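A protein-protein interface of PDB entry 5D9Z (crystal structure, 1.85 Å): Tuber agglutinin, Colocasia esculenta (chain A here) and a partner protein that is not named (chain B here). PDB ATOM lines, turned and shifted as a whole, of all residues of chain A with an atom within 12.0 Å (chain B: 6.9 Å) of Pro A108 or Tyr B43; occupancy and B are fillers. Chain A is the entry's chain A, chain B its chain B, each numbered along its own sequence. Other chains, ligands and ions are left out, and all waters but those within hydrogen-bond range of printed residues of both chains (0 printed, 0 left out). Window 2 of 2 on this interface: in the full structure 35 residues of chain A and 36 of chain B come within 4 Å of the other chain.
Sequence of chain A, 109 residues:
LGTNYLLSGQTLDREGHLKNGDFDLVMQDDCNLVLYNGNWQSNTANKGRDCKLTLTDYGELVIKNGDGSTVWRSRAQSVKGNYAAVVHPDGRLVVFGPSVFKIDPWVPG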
ATOM      1  N   LYS A 102      -1.768  14.903   8.596  1.00  0.00           N
ATOM      2  CA  LYS A 102      -1.445  16.322   8.394  1.00  0.00           C
ATOM      3  C   LYS A 102      -0.143  16.439   7.594  1.00  0.00           C
ATOM      4  O   LYS A 102       0.846  15.796   7.938  1.00  0.00           O
ATOM      5  CB  LYS A 102      -1.276  16.988   9.774  1.00  0.00           C
ATOM      6  CG  LYS A 102      -1.598  18.488   9.872  1.00  0.00           C
ATOM      7  CD  LYS A 102      -1.829  18.954  11.348  1.00  0.00           C
ATOM      8  CE  LYS A 102      -3.036  18.257  12.040  1.00  0.00           C
ATOM      9  NZ  LYS A 102      -4.284  19.099  12.183  1.00  0.00           N
ATOM     10  N   ILE A 103      -0.125  17.230   6.524  1.00  0.00           N
ATOM     11  CA  ILE A 103       1.144  17.516   5.861  1.00  0.00           C
ATOM     12  C   ILE A 103       1.462  18.975   6.096  1.00  0.00           C
ATOM     13  O   ILE A 103       0.631  19.841   5.841  1.00  0.00           O
ATOM     14  CB  ILE A 103       1.146  17.183   4.360  1.00  0.00           C
ATOM     15  CG1 ILE A 103       1.302  15.680   4.150  1.00  0.00           C
ATOM     16  CG2 ILE A 103       2.285  17.893   3.669  1.00  0.00           C
ATOM     17  CD1 ILE A 103       0.982  15.243   2.756  1.00  0.00           C
ATOM     18  N   ASP A 104       2.662  19.234   6.604  1.00  0.00           N
ATOM     19  CA  ASP A 104       3.027  20.549   7.112  1.00  0.00           C
ATOM     20  C   ASP A 104       4.213  21.083   6.342  1.00  0.00           C
ATOM     21  O   ASP A 104       5.342  20.635   6.532  1.00  0.00           O
ATOM     22  CB  ASP A 104       3.382  20.442   8.596  1.00  0.00           C
ATOM     23  CG  ASP A 104       3.655  21.789   9.248  1.00  0.00           C
ATOM     24  OD1 ASP A 104       3.919  22.787   8.538  1.00  0.00           O
ATOM     25  OD2 ASP A 104       3.616  21.828  10.495  1.00  0.00           O
ATOM     26  N   PRO A 105       3.962  22.061   5.476  1.00  0.00           N
ATOM     27  CA  PRO A 105       5.003  22.610   4.616  1.00  0.00           C
ATOM     28  C   PRO A 105       5.675  23.781   5.298  1.00  0.00           C
ATOM     29  O   PRO A 105       6.327  24.596   4.638  1.00  0.00           O
ATOM     30  CB  PRO A 105       4.202  23.117   3.426  1.00  0.00           C
ATOM     31  CG  PRO A 105       2.921  23.609   4.054  1.00  0.00           C
ATOM     32  CD  PRO A 105       2.646  22.657   5.201  1.00  0.00           C
ATOM     33  N   TRP A 106       5.501  23.882   6.608  1.00  0.00           N
ATOM     34  CA  TRP A 106       6.139  24.960   7.346  1.00  0.00           C
ATOM     35  C   TRP A 106       7.327  24.481   8.171  1.00  0.00           C
ATOM     36  O   TRP A 106       8.356  25.136   8.190  1.00  0.00           O
ATOM     37  CB  TRP A 106       5.137  25.659   8.236  1.00  0.00           C
ATOM     38  CG  TRP A 106       3.874  26.003   7.546  1.00  0.00           C
ATOM     39  CD1 TRP A 106       2.679  25.372   7.665  1.00  0.00           C
ATOM     40  CD2 TRP A 106       3.668  27.085   6.645  1.00  0.00           C
ATOM     41  NE1 TRP A 106       1.736  25.993   6.888  1.00  0.00           N
ATOM     42  CE2 TRP A 106       2.320  27.051   6.251  1.00  0.00           C
ATOM     43  CE3 TRP A 106       4.494  28.079   6.131  1.00  0.00           C
ATOM     44  CZ2 TRP A 106       1.781  27.971   5.362  1.00  0.00           C
ATOM     45  CZ3 TRP A 106       3.961  28.992   5.250  1.00  0.00           C
ATOM     46  CH2 TRP A 106       2.616  28.935   4.872  1.00  0.00           C
ATOM     47  N   VAL A 107       7.160  23.364   8.879  1.00  0.00           N
ATOM     48  CA  VAL A 107       8.278  22.669   9.525  1.00  0.00           C
ATOM     49  C   VAL A 107       9.048  21.880   8.427  1.00  0.00           C
ATOM     50  O   VAL A 107       8.440  21.470   7.438  1.00  0.00           O
ATOM     51  CB  VAL A 107       7.781  21.792  10.720  1.00  0.00           C
ATOM     52  CG1 VAL A 107       7.004  22.650  11.710  1.00  0.00           C
ATOM     53  CG2 VAL A 107       6.909  20.653  10.240  1.00  0.00           C
ATOM     54  N   PRO A 108      10.385  21.699   8.569  1.00  0.00           N
ATOM     55  CA  PRO A 108      11.203  21.159   7.461  1.00  0.00           C
ATOM     56  C   PRO A 108      11.126  19.645   7.291  1.00  0.00           C
ATOM     57  O   PRO A 108      10.511  18.983   8.128  1.00  0.00           O
ATOM     58  CB  PRO A 108      12.624  21.572   7.849  1.00  0.00           C
ATOM     59  CG  PRO A 108      12.600  21.538   9.352  1.00  0.00           C
ATOM     60  CD  PRO A 108      11.207  21.995   9.757  1.00  0.00           C
ATOM     61  N   GLY A 109      11.743  19.112   6.232  1.00  0.00           N
ATOM     62  CA  GLY A 109      11.705  17.683   5.958  1.00  0.00           C
ATOM     63  C   GLY A 109      12.685  16.866   6.780  1.00  0.00           C
ATOM     64  O   GLY A 109      13.448  16.059   6.248  1.00  0.00           O
ATOM     65  N   LEU B  38       4.003  18.735  -2.131  1.00  0.00           N
ATOM     66  CA  LEU B  38       3.241  19.953  -1.823  1.00  0.00           C
ATOM     67  C   LEU B  38       4.165  21.117  -2.161  1.00  0.00           C
ATOM     68  O   LEU B  38       5.325  21.105  -1.765  1.00  0.00           O
ATOM     69  CB  LEU B  38       2.815  19.978  -0.353  1.00  0.00           C
ATOM     70  CG  LEU B  38       2.008  21.122   0.251  1.00  0.00           C
ATOM     71  CD1 LEU B  38       1.062  21.695  -0.752  1.00  0.00           C
ATOM     72  CD2 LEU B  38       1.236  20.609   1.448  1.00  0.00           C
ATOM     73  N   GLY B  40       4.995  25.346  -2.210  1.00  0.00           N
ATOM     74  CA  GLY B  40       4.748  26.514  -1.365  1.00  0.00           C
ATOM     75  C   GLY B  40       5.193  26.366   0.095  1.00  0.00           C
ATOM     76  O   GLY B  40       6.234  25.752   0.372  1.00  0.00           O
ATOM     77  N   GLY B  41       4.412  26.927   1.029  1.00  0.00           N
ATOM     78  CA  GLY B  41       4.692  26.818   2.460  1.00  0.00           C
ATOM     79  C   GLY B  41       5.995  27.499   2.837  1.00  0.00           C
ATOM     80  O   GLY B  41       6.437  28.409   2.136  1.00  0.00           O
ATOM     81  N   LYS B  42       6.622  27.079   3.932  1.00  0.00           N
ATOM     82  CA  LYS B  42       7.929  27.633   4.277  1.00  0.00           C
ATOM     83  C   LYS B  42       9.008  26.690   3.794  1.00  0.00           C
ATOM     84  O   LYS B  42      10.125  27.098   3.489  1.00  0.00           O
ATOM     85  CB  LYS B  42       8.060  27.853   5.781  1.00  0.00           C
ATOM     86  CG  LYS B  42       8.806  29.135   6.184  1.00  0.00           C
ATOM     87  CD  LYS B  42       8.403  29.506   7.617  1.00  0.00           C
ATOM     88  CE  LYS B  42       9.303  30.550   8.277  1.00  0.00           C
ATOM     89  NZ  LYS B  42       8.983  30.670   9.748  1.00  0.00           N
ATOM     90  N   TYR B  43       8.653  25.418   3.718  1.00  0.00           N
ATOM     91  CA  TYR B  43       9.587  24.400   3.286  1.00  0.00           C
ATOM     92  C   TYR B  43       8.937  23.455   2.284  1.00  0.00           C
ATOM     93  O   TYR B  43       9.605  22.869   1.440  1.00  0.00           O
ATOM     94  CB  TYR B  43      10.100  23.613   4.494  1.00  0.00           C
ATOM     95  CG  TYR B  43      10.879  24.439   5.488  1.00  0.00           C
ATOM     96  CD1 TYR B  43      11.782  25.419   5.076  1.00  0.00           C
ATOM     97  CD2 TYR B  43      10.707  24.241   6.838  1.00  0.00           C
ATOM     98  CE1 TYR B  43      12.483  26.173   5.994  1.00  0.00           C
ATOM     99  CE2 TYR B  43      11.401  24.963   7.761  1.00  0.00           C
ATOM    100  CZ  TYR B  43      12.289  25.935   7.345  1.00  0.00           C
ATOM    101  OH  TYR B  43      12.978  26.671   8.287  1.00  0.00           O
ATOM    102  N   GLY B  44       7.627  23.302   2.377  1.00  0.00           N
ATOM    103  CA  GLY B  44       6.952  22.353   1.522  1.00  0.00           C
ATOM    104  C   GLY B  44       7.155  20.915   1.961  1.00  0.00           C
ATOM    105  O   GLY B  44       7.768  20.647   3.002  1.00  0.00           O
ATOM    106  N   TRP B  45       6.653  19.991   1.147  1.00  0.00           N
ATOM    107  CA  TRP B  45       6.685  18.583   1.480  1.00  0.00           C
ATOM    108  C   TRP B  45       6.899  17.751   0.243  1.00  0.00           C
ATOM    109  O   TRP B  45       6.442  18.122  -0.836  1.00  0.00           O
ATOM    110  CB  TRP B  45       5.354  18.194   2.069  1.00  0.00           C
ATOM    111  CG  TRP B  45       5.317  16.792   2.524  1.00  0.00           C
ATOM    112  CD1 TRP B  45       5.702  16.333   3.732  1.00  0.00           C
ATOM    113  CD2 TRP B  45       4.857  15.651   1.787  1.00  0.00           C
ATOM    114  NE1 TRP B  45       5.516  14.973   3.808  1.00  0.00           N
ATOM    115  CE2 TRP B  45       4.995  14.532   2.626  1.00  0.00           C
ATOM    116  CE3 TRP B  45       4.339  15.471   0.511  1.00  0.00           C
ATOM    117  CZ2 TRP B  45       4.638  13.241   2.220  1.00  0.00           C
ATOM    118  CZ3 TRP B  45       3.990  14.193   0.110  1.00  0.00           C
ATOM    119  CH2 TRP B  45       4.135  13.096   0.964  1.00  0.00           C
ATOM    120  N   GLN B  46       7.587  16.624   0.399  1.00  0.00           N
ATOM    121  CA  GLN B  46       7.666  15.621  -0.648  1.00  0.00           C
ATOM    122  C   GLN B  46       7.602  14.269   0.021  1.00  0.00           C
ATOM    123  O   GLN B  46       7.765  14.174   1.228  1.00  0.00           O
ATOM    124  CB  GLN B  46       8.946  15.765  -1.465  1.00  0.00           C
ATOM    125  CG  GLN B  46      10.203  15.350  -0.746  1.00  0.00           C
ATOM    126  CD  GLN B  46      11.430  15.556  -1.604  1.00  0.00           C
ATOM    127  OE1 GLN B  46      11.328  15.970  -2.757  1.00  0.00           O
ATOM    128  NE2 GLN B  46      12.596  15.273  -1.049  1.00  0.00           N
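The backbone carbonyl oxygen of Pro A105 sits at hydrogen-bond distance from the backbone NH of Tyr B43.
O of Pro A105 lies within hydrogen-bond range of N of Lys B42, at 2.6 Å.
The backbone NH (N) of Gly B44 lies within hydrogen-bond range of the backbone carbonyl oxygen (O) of Pro A105 (2.9 Å).
Of the printed residues of chain B, Ile A103 touches Leu B38 and Trp B45.
Printed residues of chain B within 4 Å of Val A107: Tyr B43 (3.3 Å).
Of chain B, only Tyr B43 (3.1 Å) comes within 4 Å of Pro A108.
Gly A109 touches none of the printed residues of chain B.
Of the printed residues of chain A, Leu B38 touches Ile A103 (3.7 Å).
Lys B42 touches two residues of chain A.
Tyr B43 touches just these residues of chain A: Pro A105, Trp A106, Val A107 and Pro A108.
Of chain A, only Pro A105 comes within 4 Å of Gly B44.
Printed residues of chain A within 4 Å of Trp B45: Ile A103.
The nearest residue of chain B that does not touch Pro A108 is Gly B44 (5.5 Å).
N of Leu B38 lies within hydrogen-bond range of O of Trp B45 (2.8 Å).
The backbone NH (N) of Trp A106 lies within hydrogen-bond range of the side-chain carboxylate (OD1) of Asp A104 (2.7 Å).
OD1 of Asp A104 sits at hydrogen-bond distance from N of Val A107.
Among the printed residues, no Asp or Glu carboxylate lies within 4 Å of a Lys or Arg side-chain nitrogen of the other chain.
Leu B38 touches Ile A103 (CD2 to CG2, 3.7 Å).
Ile A103 touches Trp B45 (CG2 to CG, 3.4 Å).
O of Pro A105 touches C of Gly B41 (3.4 Å).
Gly B41 touches Trp A106 (C to CZ3, 3.5 Å).
N of Lys B42 touches CE3 of Trp A106 (3.2 Å).
Tyr B43 touches Trp A106.
Tyr B43 touches Val A107.
Pro A108 touches Tyr B43.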
